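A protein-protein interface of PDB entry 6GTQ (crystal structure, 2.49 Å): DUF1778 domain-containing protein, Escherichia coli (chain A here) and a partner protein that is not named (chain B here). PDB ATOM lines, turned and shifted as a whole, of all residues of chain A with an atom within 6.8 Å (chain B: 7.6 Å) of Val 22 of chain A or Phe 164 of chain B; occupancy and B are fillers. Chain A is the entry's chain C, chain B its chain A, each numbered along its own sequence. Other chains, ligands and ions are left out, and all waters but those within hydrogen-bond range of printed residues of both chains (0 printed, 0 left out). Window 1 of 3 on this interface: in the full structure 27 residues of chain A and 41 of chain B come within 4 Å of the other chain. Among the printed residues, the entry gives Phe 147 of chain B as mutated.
OG of Ser 169 of chain B is in hydrogen-bond range of O of Pro 30 of chain A, at 2.8 Å.
The guanidinium group (NH1) of Arg 21 of chain A sits at hydrogen-bond distance from the backbone carbonyl oxygen (O) of Pro 154 of chain B (2.8 Å).
The backbone NH of Ile 153 of chain B lies within hydrogen-bond range of the backbone carbonyl oxygen of Phe 164 of chain B (2.8 Å).
The backbone carbonyl oxygen of Phe 72 of chain B lies within hydrogen-bond range of the backbone NH of Ile 91 of chain B (2.8 Å).
The backbone carbonyl oxygen (O) of His 132 of chain B lies within hydrogen-bond range of the backbone NH (N) of Thr 167 of chain B (3.2 Å).
The side-chain hydroxyl (OG) of Ser 27 of chain A sits at hydrogen-bond distance from the backbone carbonyl oxygen (O) of Met 23 of chain A (3.2 Å).
The backbone carbonyl oxygen of Pro 92 of chain B lies within hydrogen-bond range of the backbone NH of His 132 of chain B (3.0 Å).
The side-chain hydroxyl of Ser 93 of chain B lies within hydrogen-bond range of the backbone carbonyl oxygen of Ile 91 of chain B (3.5 Å).
Among the printed residues, pairs that only touch across the chains: Asn 15 of chain A with Phe 72 of chain B (3.8 Å), Ser 18 of chain A with Leu 155 of chain B (3.5 Å), Trp 19 of chain A with Phe 72 of chain B (3.9 Å), Trp 19 of chain A with Ile 91 of chain B (3.6 Å), Val 22 of chain A with Ile 91 of chain B (3.6 Å), Val 22 of chain A with Leu 155 of chain B (3.6 Å), Val 22 of chain A with Phe 164 of chain B (3.6 Å), Met 23 of chain A with Ile 91 of chain B (3.7 Å), Ala 25 of chain A with Ile 153 of chain B (3.8 Å), Ala 25 of chain A with Phe 164 of chain B (3.8 Å), Ala 25 of chain A with Pro 166 of chain B (3.3 Å), Leu 26 of chain A with His 132 of chain B (3.4 Å), Leu 26 of chain A with Phe 164 of chain B (3.9 Å), Leu 26 of chain A with Pro 166 of chain B (3.95 Å), Pro 30 of chain A with Ile 153 of chain B (3.7 Å) and Pro 30 of chain A with Pro 166 of chain B (3.8 Å).
Of chain B, only Ile 91, Leu 155 and Phe 164 come within 4 Å of Val 22 of chain A.
Phe 164 of chain B touches just these residues of chain A: Val 22, Ala 25 and Leu 26.
Of the printed residues of chain B, Leu 26 of chain A touches His 132 (3.4 Å), Phe 164 (3.9 Å) and Pro 166 (3.95 Å).
Of the printed residues of chain A, His 132 of chain B touches Leu 26 (3.4 Å).
Of the 23 printed residues of chain B, 9 touch a printed residue of chain A.
Printed residues of chain B that touch a printed residue of chain A: Phe 72, Ile 91, His 132, Ile 153, Pro 154, Leu 155, Phe 164, Pro 166 and Ser 169.
Hydrophobic or aromatic side chains of chain B that line the printed part of chain A: Phe 72, Ile 91, Ile 153, Leu 155, Phe 164 and Pro 166.
Along chain B the printed residues that touch a printed residue of chain A span positions 72 to 169.
Hydrophobic or aromatic side chains of chain A within 4 Å of the printed part of chain B: Trp 19, Val 22, Met 23, Ala 25, Leu 26 and Pro 30.
Among the printed residues, 18 pairs touch across the chains.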
ATOM      1  N   ASN A  15       8.956  23.376 -19.917  1.00  0.00           N
ATOM      2  CA  ASN A  15       9.006  24.278 -21.081  1.00  0.00           C
ATOM      3  C   ASN A  15       9.229  25.791 -20.884  1.00  0.00           C
ATOM      4  O   ASN A  15       9.071  26.264 -19.804  1.00  0.00           O
ATOM      5  CB  ASN A  15       7.702  24.084 -21.849  1.00  0.00           C
ATOM      6  CG  ASN A  15       7.539  22.694 -22.413  1.00  0.00           C
ATOM      7  OD1 ASN A  15       8.487  21.994 -22.584  1.00  0.00           O
ATOM      8  ND2 ASN A  15       6.329  22.317 -22.733  1.00  0.00           N
ATOM      9  N   GLU A  17       9.798  28.842 -24.235  1.00  0.00           N
ATOM     10  CA  GLU A  17       9.226  29.322 -25.490  1.00  0.00           C
ATOM     11  C   GLU A  17       8.813  28.067 -26.312  1.00  0.00           C
ATOM     12  O   GLU A  17       8.255  28.154 -27.361  1.00  0.00           O
ATOM     13  CB  GLU A  17      10.248  30.111 -26.259  1.00  0.00           C
ATOM     14  CG  GLU A  17      10.775  29.427 -27.508  1.00  0.00           C
ATOM     15  CD  GLU A  17      10.454  30.179 -28.778  1.00  0.00           C
ATOM     16  OE1 GLU A  17      10.210  31.366 -28.650  1.00  0.00           O
ATOM     17  OE2 GLU A  17      10.418  29.610 -29.878  1.00  0.00           O
ATOM     18  N   SER A  18       9.188  26.899 -25.810  1.00  0.00           N
ATOM     19  CA  SER A  18       8.888  25.603 -26.280  1.00  0.00           C
ATOM     20  C   SER A  18       7.445  25.371 -25.981  1.00  0.00           C
ATOM     21  O   SER A  18       6.822  24.583 -26.573  1.00  0.00           O
ATOM     22  CB  SER A  18       9.758  24.655 -25.516  1.00  0.00           C
ATOM     23  OG  SER A  18      11.059  24.774 -25.969  1.00  0.00           O
ATOM     24  N   TRP A  19       6.973  26.070 -24.981  1.00  0.00           N
ATOM     25  CA  TRP A  19       5.601  26.049 -24.516  1.00  0.00           C
ATOM     26  C   TRP A  19       4.667  26.587 -25.599  1.00  0.00           C
ATOM     27  O   TRP A  19       3.622  25.979 -25.838  1.00  0.00           O
ATOM     28  CB  TRP A  19       5.470  26.864 -23.222  1.00  0.00           C
ATOM     29  CG  TRP A  19       4.060  26.939 -22.714  1.00  0.00           C
ATOM     30  CD1 TRP A  19       3.172  27.957 -22.902  1.00  0.00           C
ATOM     31  CD2 TRP A  19       3.351  25.909 -22.019  1.00  0.00           C
ATOM     32  NE1 TRP A  19       1.962  27.638 -22.336  1.00  0.00           N
ATOM     33  CE2 TRP A  19       2.043  26.386 -21.785  1.00  0.00           C
ATOM     34  CE3 TRP A  19       3.703  24.631 -21.550  1.00  0.00           C
ATOM     35  CZ2 TRP A  19       1.081  25.629 -21.111  1.00  0.00           C
ATOM     36  CZ3 TRP A  19       2.756  23.893 -20.852  1.00  0.00           C
ATOM     37  CH2 TRP A  19       1.459  24.383 -20.654  1.00  0.00           C
ATOM     38  N   THR A  20       5.038  27.728 -26.245  1.00  0.00           N
ATOM     39  CA  THR A  20       4.249  28.337 -27.317  1.00  0.00           C
ATOM     40  C   THR A  20       4.210  27.413 -28.545  1.00  0.00           C
ATOM     41  O   THR A  20       3.163  27.308 -29.173  1.00  0.00           O
ATOM     42  CB  THR A  20       4.696  29.775 -27.650  1.00  0.00           C
ATOM     43  OG1 THR A  20       6.029  29.782 -28.157  1.00  0.00           O
ATOM     44  CG2 THR A  20       4.553  30.740 -26.480  1.00  0.00           C
ATOM     45  N   ARG A  21       5.331  26.714 -28.850  1.00  0.00           N
ATOM     46  CA  ARG A  21       5.451  25.763 -29.960  1.00  0.00           C
ATOM     47  C   ARG A  21       4.489  24.606 -29.781  1.00  0.00           C
ATOM     48  O   ARG A  21       3.852  24.202 -30.752  1.00  0.00           O
ATOM     49  CB  ARG A  21       6.891  25.245 -30.104  1.00  0.00           C
ATOM     50  CG  ARG A  21       7.849  26.304 -30.613  1.00  0.00           C
ATOM     51  CD  ARG A  21       9.202  25.749 -30.949  1.00  0.00           C
ATOM     52  NE  ARG A  21      10.010  26.760 -31.626  1.00  0.00           N
ATOM     53  CZ  ARG A  21      11.252  26.570 -32.055  1.00  0.00           C
ATOM     54  NH1 ARG A  21      11.853  25.401 -31.876  1.00  0.00           N
ATOM     55  NH2 ARG A  21      11.905  27.548 -32.666  1.00  0.00           N
ATOM     56  N   VAL A  22       4.358  24.100 -28.534  1.00  0.00           N
ATOM     57  CA  VAL A  22       3.444  23.017 -28.152  1.00  0.00           C
ATOM     58  C   VAL A  22       2.005  23.531 -28.194  1.00  0.00           C
ATOM     59  O   VAL A  22       1.157  22.858 -28.770  1.00  0.00           O
ATOM     60  CB  VAL A  22       3.809  22.337 -26.802  1.00  0.00           C
ATOM     61  CG1 VAL A  22       2.759  21.302 -26.404  1.00  0.00           C
ATOM     62  CG2 VAL A  22       5.183  21.672 -26.872  1.00  0.00           C
ATOM     63  N   MET A  23       1.741  24.741 -27.650  1.00  0.00           N
ATOM     64  CA  MET A  23       0.419  25.377 -27.685  1.00  0.00           C
ATOM     65  C   MET A  23      -0.070  25.576 -29.114  1.00  0.00           C
ATOM     66  O   MET A  23      -1.248  25.332 -29.391  1.00  0.00           O
ATOM     67  CB  MET A  23       0.408  26.723 -26.931  1.00  0.00           C
ATOM     68  CG  MET A  23       0.432  26.600 -25.426  1.00  0.00           C
ATOM     69  SD  MET A  23      -0.724  25.404 -24.707  1.00  0.00           S
ATOM     70  CE  MET A  23       0.398  24.063 -24.331  1.00  0.00           C
ATOM     71  N   ASP A  24       0.844  26.005 -30.017  1.00  0.00           N
ATOM     72  CA  ASP A  24       0.579  26.233 -31.441  1.00  0.00           C
ATOM     73  C   ASP A  24       0.339  24.934 -32.180  1.00  0.00           C
ATOM     74  O   ASP A  24      -0.467  24.916 -33.105  1.00  0.00           O
ATOM     75  CB  ASP A  24       1.719  27.010 -32.106  1.00  0.00           C
ATOM     76  CG  ASP A  24       1.846  28.459 -31.670  1.00  0.00           C
ATOM     77  OD1 ASP A  24       1.151  28.860 -30.703  1.00  0.00           O
ATOM     78  OD2 ASP A  24       2.654  29.187 -32.277  1.00  0.00           O
ATOM     79  N   ALA A  25       1.034  23.852 -31.768  1.00  0.00           N
ATOM     80  CA  ALA A  25       0.888  22.514 -32.342  1.00  0.00           C
ATOM     81  C   ALA A  25      -0.490  21.955 -31.967  1.00  0.00           C
ATOM     82  O   ALA A  25      -1.094  21.251 -32.762  1.00  0.00           O
ATOM     83  CB  ALA A  25       1.982  21.599 -31.822  1.00  0.00           C
ATOM     84  N   LEU A  26      -0.995  22.300 -30.775  1.00  0.00           N
ATOM     85  CA  LEU A  26      -2.306  21.861 -30.304  1.00  0.00           C
ATOM     86  C   LEU A  26      -3.454  22.585 -31.025  1.00  0.00           C
ATOM     87  O   LEU A  26      -4.457  21.946 -31.356  1.00  0.00           O
ATOM     88  CB  LEU A  26      -2.432  22.000 -28.770  1.00  0.00           C
ATOM     89  CG  LEU A  26      -1.538  21.077 -27.921  1.00  0.00           C
ATOM     90  CD1 LEU A  26      -1.558  21.498 -26.462  1.00  0.00           C
ATOM     91  CD2 LEU A  26      -1.942  19.613 -28.049  1.00  0.00           C
ATOM     92  N   SER A  27      -3.304  23.898 -31.273  1.00  0.00           N
ATOM     93  CA  SER A  27      -4.325  24.700 -31.938  1.00  0.00           C
ATOM     94  C   SER A  27      -4.250  24.573 -33.449  1.00  0.00           C
ATOM     95  O   SER A  27      -5.250  24.813 -34.125  1.00  0.00           O
ATOM     96  CB  SER A  27      -4.247  26.161 -31.502  1.00  0.00           C
ATOM     97  OG  SER A  27      -2.978  26.736 -31.756  1.00  0.00           O
ATOM     98  N   PRO A  30      -0.111  19.521 -36.941  1.00  0.00           N
ATOM     99  CA  PRO A  30       0.521  19.212 -38.233  1.00  0.00           C
ATOM    100  C   PRO A  30      -0.172  18.093 -39.010  1.00  0.00           C
ATOM    101  O   PRO A  30      -0.738  17.185 -38.414  1.00  0.00           O
ATOM    102  CB  PRO A  30       1.955  18.833 -37.849  1.00  0.00           C
ATOM    103  CG  PRO A  30       1.895  18.460 -36.426  1.00  0.00           C
ATOM    104  CD  PRO A  30       0.824  19.284 -35.815  1.00  0.00           C
ATOM    105  N   PHE B  72       3.789  17.948 -19.328  1.00  0.00           N
ATOM    106  CA  PHE B  72       4.591  19.092 -19.706  1.00  0.00           C
ATOM    107  C   PHE B  72       4.009  20.314 -19.013  1.00  0.00           C
ATOM    108  O   PHE B  72       2.793  20.505 -19.008  1.00  0.00           O
ATOM    109  CB  PHE B  72       4.608  19.266 -21.228  1.00  0.00           C
ATOM    110  N   ILE B  91       0.170  19.739 -19.350  1.00  0.00           N
ATOM    111  CA  ILE B  91      -0.155  18.915 -20.530  1.00  0.00           C
ATOM    112  C   ILE B  91      -0.064  17.412 -20.193  1.00  0.00           C
ATOM    113  O   ILE B  91       1.046  16.883 -20.280  1.00  0.00           O
ATOM    114  CB  ILE B  91       0.724  19.216 -21.815  1.00  0.00           C
ATOM    115  CG1 ILE B  91       0.811  20.715 -22.151  1.00  0.00           C
ATOM    116  CG2 ILE B  91       0.254  18.400 -23.054  1.00  0.00           C
ATOM    117  CD1 ILE B  91       2.060  21.072 -22.908  1.00  0.00           C
ATOM    118  N   PRO B  92      -1.175  16.676 -19.908  1.00  0.00           N
ATOM    119  CA  PRO B  92      -1.055  15.213 -19.752  1.00  0.00           C
ATOM    120  C   PRO B  92      -0.592  14.614 -21.079  1.00  0.00           C
ATOM    121  O   PRO B  92      -1.193  14.887 -22.131  1.00  0.00           O
ATOM    122  CB  PRO B  92      -2.465  14.763 -19.378  1.00  0.00           C
ATOM    123  CG  PRO B  92      -3.368  15.852 -19.857  1.00  0.00           C
ATOM    124  CD  PRO B  92      -2.579  17.123 -19.790  1.00  0.00           C
ATOM    125  N   SER B  93       0.547  13.904 -21.045  1.00  0.00           N
ATOM    126  CA  SER B  93       1.170  13.331 -22.246  1.00  0.00           C
ATOM    127  C   SER B  93       1.843  11.967 -22.008  1.00  0.00           C
ATOM    128  O   SER B  93       1.741  11.394 -20.931  1.00  0.00           O
ATOM    129  CB  SER B  93       2.178  14.319 -22.834  1.00  0.00           C
ATOM    130  OG  SER B  93       3.164  14.663 -21.877  1.00  0.00           O
ATOM    131  N   VAL B  94       2.492  11.437 -23.048  1.00  0.00           N
ATOM    132  CA  VAL B  94       3.259  10.200 -22.999  1.00  0.00           C
ATOM    133  C   VAL B  94       4.617  10.501 -23.618  1.00  0.00           C
ATOM    134  O   VAL B  94       4.690  11.170 -24.650  1.00  0.00           O
ATOM    135  CB  VAL B  94       2.556   9.019 -23.717  1.00  0.00           C
ATOM    136  CG1 VAL B  94       3.438   7.766 -23.696  1.00  0.00           C
ATOM    137  CG2 VAL B  94       1.182   8.732 -23.099  1.00  0.00           C
ATOM    138  N   HIS B 132      -3.063  14.588 -24.407  1.00  0.00           N
ATOM    139  CA  HIS B 132      -2.973  15.562 -25.498  1.00  0.00           C
ATOM    140  C   HIS B 132      -1.809  15.492 -26.474  1.00  0.00           C
ATOM    141  O   HIS B 132      -1.786  16.221 -27.458  1.00  0.00           O
ATOM    142  CB  HIS B 132      -3.130  16.972 -24.939  1.00  0.00           C
ATOM    143  CG  HIS B 132      -4.355  17.136 -24.102  1.00  0.00           C
ATOM    144  ND1 HIS B 132      -4.319  17.608 -22.811  1.00  0.00           N
ATOM    145  CD2 HIS B 132      -5.652  16.857 -24.365  1.00  0.00           C
ATOM    146  CE1 HIS B 132      -5.543  17.628 -22.318  1.00  0.00           C
ATOM    147  NE2 HIS B 132      -6.370  17.175 -23.240  1.00  0.00           N
ATOM    148  N   GLY B 133      -0.843  14.629 -26.212  1.00  0.00           N
ATOM    149  CA  GLY B 133       0.284  14.506 -27.117  1.00  0.00           C
ATOM    150  C   GLY B 133       1.342  13.503 -26.743  1.00  0.00           C
ATOM    151  O   GLY B 133       1.281  12.862 -25.689  1.00  0.00           O
ATOM    152  N   LEU B 134       2.321  13.382 -27.646  1.00  0.00           N
ATOM    153  CA  LEU B 134       3.477  12.505 -27.555  1.00  0.00           C
ATOM    154  C   LEU B 134       4.754  13.333 -27.659  1.00  0.00           C
ATOM    155  O   LEU B 134       4.931  14.102 -28.619  1.00  0.00           O
ATOM    156  CB  LEU B 134       3.442  11.399 -28.654  1.00  0.00           C
ATOM    157  CG  LEU B 134       4.668  10.471 -28.758  1.00  0.00           C
ATOM    158  CD1 LEU B 134       4.806   9.548 -27.537  1.00  0.00           C
ATOM    159  CD2 LEU B 134       4.632   9.648 -30.029  1.00  0.00           C
ATOM    160  N   PHE B 135       5.636  13.162 -26.651  1.00  0.00           N
ATOM    161  CA  PHE B 135       6.960  13.775 -26.583  1.00  0.00           C
ATOM    162  C   PHE B 135       7.975  12.701 -26.884  1.00  0.00           C
ATOM    163  O   PHE B 135       7.748  11.535 -26.581  1.00  0.00           O
ATOM    164  CB  PHE B 135       7.233  14.396 -25.208  1.00  0.00           C
ATOM    165  CG  PHE B 135       6.480  15.678 -24.968  1.00  0.00           C
ATOM    166  CD1 PHE B 135       5.212  15.663 -24.405  1.00  0.00           C
ATOM    167  CD2 PHE B 135       7.031  16.904 -25.326  1.00  0.00           C
ATOM    168  CE1 PHE B 135       4.515  16.858 -24.184  1.00  0.00           C
ATOM    169  CE2 PHE B 135       6.332  18.092 -25.114  1.00  0.00           C
ATOM    170  CZ  PHE B 135       5.082  18.061 -24.540  1.00  0.00           C
ATOM    171  N   VAL B 136       9.088  13.082 -27.496  1.00  0.00           N
ATOM    172  CA  VAL B 136      10.127  12.129 -27.857  1.00  0.00           C
ATOM    173  C   VAL B 136      11.506  12.672 -27.484  1.00  0.00           C
ATOM    174  O   VAL B 136      11.705  13.885 -27.467  1.00  0.00           O
ATOM    175  CB  VAL B 136       9.979  11.681 -29.336  1.00  0.00           C
ATOM    176  CG1 VAL B 136      10.642  12.644 -30.312  1.00  0.00           C
ATOM    177  CG2 VAL B 136      10.490  10.273 -29.529  1.00  0.00           C
ATOM    178  N   PHE B 147      13.069  12.352 -36.316  1.00  0.00           N
ATOM    179  CA  PHE B 147      11.812  12.741 -35.692  1.00  0.00           C
ATOM    180  C   PHE B 147      11.175  13.936 -36.396  1.00  0.00           C
ATOM    181  O   PHE B 147       9.956  13.939 -36.552  1.00  0.00           O
ATOM    182  CB  PHE B 147      11.956  12.933 -34.174  1.00  0.00           C
ATOM    183  CG  PHE B 147      12.128  11.614 -33.449  1.00  0.00           C
ATOM    184  CD1 PHE B 147      11.150  10.626 -33.522  1.00  0.00           C
ATOM    185  CD2 PHE B 147      13.259  11.368 -32.678  1.00  0.00           C
ATOM    186  CE1 PHE B 147      11.319   9.401 -32.873  1.00  0.00           C
ATOM    187  CE2 PHE B 147      13.426  10.145 -32.023  1.00  0.00           C
ATOM    188  CZ  PHE B 147      12.461   9.165 -32.133  1.00  0.00           C
ATOM    189  N   GLY B 151       7.378  14.499 -38.620  1.00  0.00           N
ATOM    190  CA  GLY B 151       6.475  15.605 -38.314  1.00  0.00           C
ATOM    191  C   GLY B 151       6.479  16.123 -36.888  1.00  0.00           C
ATOM    192  O   GLY B 151       5.617  16.935 -36.526  1.00  0.00           O
ATOM    193  N   PHE B 152       7.435  15.663 -36.058  1.00  0.00           N
ATOM    194  CA  PHE B 152       7.539  16.127 -34.671  1.00  0.00           C
ATOM    195  C   PHE B 152       8.043  17.577 -34.643  1.00  0.00           C
ATOM    196  O   PHE B 152       8.903  17.945 -35.445  1.00  0.00           O
ATOM    197  CB  PHE B 152       8.450  15.213 -33.851  1.00  0.00           C
ATOM    198  CG  PHE B 152       7.864  13.890 -33.424  1.00  0.00           C
ATOM    199  CD1 PHE B 152       7.768  12.829 -34.319  1.00  0.00           C
ATOM    200  CD2 PHE B 152       7.497  13.670 -32.102  1.00  0.00           C
ATOM    201  CE1 PHE B 152       7.274  11.591 -33.910  1.00  0.00           C
ATOM    202  CE2 PHE B 152       6.980  12.436 -31.696  1.00  0.00           C
ATOM    203  CZ  PHE B 152       6.883  11.402 -32.600  1.00  0.00           C
ATOM    204  N   ILE B 153       7.459  18.408 -33.771  1.00  0.00           N
ATOM    205  CA  ILE B 153       7.827  19.813 -33.651  1.00  0.00           C
ATOM    206  C   ILE B 153       9.027  19.906 -32.725  1.00  0.00           C
ATOM    207  O   ILE B 153       8.929  19.470 -31.581  1.00  0.00           O
ATOM    208  CB  ILE B 153       6.622  20.719 -33.215  1.00  0.00           C
ATOM    209  CG1 ILE B 153       5.584  20.855 -34.352  1.00  0.00           C
ATOM    210  CG2 ILE B 153       7.074  22.115 -32.752  1.00  0.00           C
ATOM    211  CD1 ILE B 153       4.395  19.955 -34.210  1.00  0.00           C
ATOM    212  N   PRO B 154      10.175  20.450 -33.191  1.00  0.00           N
ATOM    213  CA  PRO B 154      11.342  20.546 -32.296  1.00  0.00           C
ATOM    214  C   PRO B 154      11.206  21.641 -31.238  1.00  0.00           C
ATOM    215  O   PRO B 154      10.831  22.779 -31.546  1.00  0.00           O
ATOM    216  CB  PRO B 154      12.509  20.798 -33.254  1.00  0.00           C
ATOM    217  CG  PRO B 154      11.896  21.459 -34.435  1.00  0.00           C
ATOM    218  CD  PRO B 154      10.469  21.007 -34.533  1.00  0.00           C
ATOM    219  N   LEU B 155      11.490  21.277 -29.980  1.00  0.00           N
ATOM    220  CA  LEU B 155      11.473  22.209 -28.850  1.00  0.00           C
ATOM    221  C   LEU B 155      12.852  22.848 -28.709  1.00  0.00           C
ATOM    222  O   LEU B 155      13.827  22.313 -29.236  1.00  0.00           O
ATOM    223  CB  LEU B 155      10.974  21.542 -27.554  1.00  0.00           C
ATOM    224  CG  LEU B 155       9.553  20.975 -27.612  1.00  0.00           C
ATOM    225  CD1 LEU B 155       9.122  20.450 -26.262  1.00  0.00           C
ATOM    226  CD2 LEU B 155       8.561  21.998 -28.151  1.00  0.00           C
ATOM    227  N   ALA B 162      13.921  17.438 -26.925  1.00  0.00           N
ATOM    228  CA  ALA B 162      12.532  16.996 -27.006  1.00  0.00           C
ATOM    229  C   ALA B 162      11.828  17.511 -28.261  1.00  0.00           C
ATOM    230  O   ALA B 162      12.092  18.622 -28.726  1.00  0.00           O
ATOM    231  CB  ALA B 162      11.765  17.398 -25.753  1.00  0.00           C
ATOM    232  N   LEU B 163      10.959  16.669 -28.824  1.00  0.00           N
ATOM    233  CA  LEU B 163      10.137  16.967 -29.993  1.00  0.00           C
ATOM    234  C   LEU B 163       8.704  16.580 -29.650  1.00  0.00           C
ATOM    235  O   LEU B 163       8.489  15.574 -28.957  1.00  0.00           O
ATOM    236  CB  LEU B 163      10.609  16.209 -31.237  1.00  0.00           C
ATOM    237  CG  LEU B 163      11.959  16.601 -31.797  1.00  0.00           C
ATOM    238  CD1 LEU B 163      12.977  15.508 -31.535  1.00  0.00           C
ATOM    239  CD2 LEU B 163      11.858  16.906 -33.277  1.00  0.00           C
ATOM    240  N   PHE B 164       7.730  17.371 -30.123  1.00  0.00           N
ATOM    241  CA  PHE B 164       6.324  17.142 -29.804  1.00  0.00           C
ATOM    242  C   PHE B 164       5.422  16.814 -30.999  1.00  0.00           C
ATOM    243  O   PHE B 164       5.526  17.450 -32.049  1.00  0.00           O
ATOM    244  CB  PHE B 164       5.760  18.348 -29.026  1.00  0.00           C
ATOM    245  CG  PHE B 164       4.297  18.247 -28.673  1.00  0.00           C
ATOM    246  CD1 PHE B 164       3.857  17.350 -27.709  1.00  0.00           C
ATOM    247  CD2 PHE B 164       3.354  19.048 -29.310  1.00  0.00           C
ATOM    248  CE1 PHE B 164       2.505  17.269 -27.374  1.00  0.00           C
ATOM    249  CE2 PHE B 164       1.999  18.942 -28.996  1.00  0.00           C
ATOM    250  CZ  PHE B 164       1.585  18.058 -28.025  1.00  0.00           C
ATOM    251  N   PHE B 165       4.493  15.854 -30.794  1.00  0.00           N
ATOM    252  CA  PHE B 165       3.470  15.471 -31.760  1.00  0.00           C
ATOM    253  C   PHE B 165       2.087  15.419 -31.067  1.00  0.00           C
ATOM    254  O   PHE B 165       1.907  14.641 -30.124  1.00  0.00           O
ATOM    255  CB  PHE B 165       3.811  14.148 -32.446  1.00  0.00           C
ATOM    256  CG  PHE B 165       3.221  14.001 -33.827  1.00  0.00           C
ATOM    257  CD1 PHE B 165       3.725  14.728 -34.900  1.00  0.00           C
ATOM    258  CD2 PHE B 165       2.181  13.110 -34.064  1.00  0.00           C
ATOM    259  CE1 PHE B 165       3.189  14.576 -36.178  1.00  0.00           C
ATOM    260  CE2 PHE B 165       1.673  12.930 -35.351  1.00  0.00           C
ATOM    261  CZ  PHE B 165       2.173  13.668 -36.397  1.00  0.00           C
ATOM    262  N   PRO B 166       1.111  16.262 -31.483  1.00  0.00           N
ATOM    263  CA  PRO B 166      -0.202  16.248 -30.814  1.00  0.00           C
ATOM    264  C   PRO B 166      -1.071  15.029 -31.135  1.00  0.00           C
ATOM    265  O   PRO B 166      -0.891  14.403 -32.173  1.00  0.00           O
ATOM    266  CB  PRO B 166      -0.859  17.568 -31.256  1.00  0.00           C
ATOM    267  CG  PRO B 166       0.149  18.270 -32.104  1.00  0.00           C
ATOM    268  CD  PRO B 166       1.148  17.265 -32.562  1.00  0.00           C
ATOM    269  N   THR B 167      -2.027  14.700 -30.239  1.00  0.00           N
ATOM    270  CA  THR B 167      -2.943  13.564 -30.429  1.00  0.00           C
ATOM    271  C   THR B 167      -3.839  13.754 -31.660  1.00  0.00           C
ATOM    272  O   THR B 167      -4.111  12.778 -32.361  1.00  0.00           O
ATOM    273  CB  THR B 167      -3.733  13.259 -29.151  1.00  0.00           C
ATOM    274  OG1 THR B 167      -2.801  13.055 -28.096  1.00  0.00           O
ATOM    275  CG2 THR B 167      -4.603  12.010 -29.280  1.00  0.00           C
ATOM    276  N   SER B 169      -3.098  15.100 -34.507  1.00  0.00           N
ATOM    277  CA  SER B 169      -2.311  14.712 -35.686  1.00  0.00           C
ATOM    278  C   SER B 169      -2.241  13.191 -35.796  1.00  0.00           C
ATOM    279  O   SER B 169      -2.224  12.667 -36.901  1.00  0.00           O
ATOM    280  CB  SER B 169      -0.905  15.289 -35.610  1.00  0.00           C
ATOM    281  OG  SER B 169      -0.937  16.704 -35.640  1.00  0.00           O
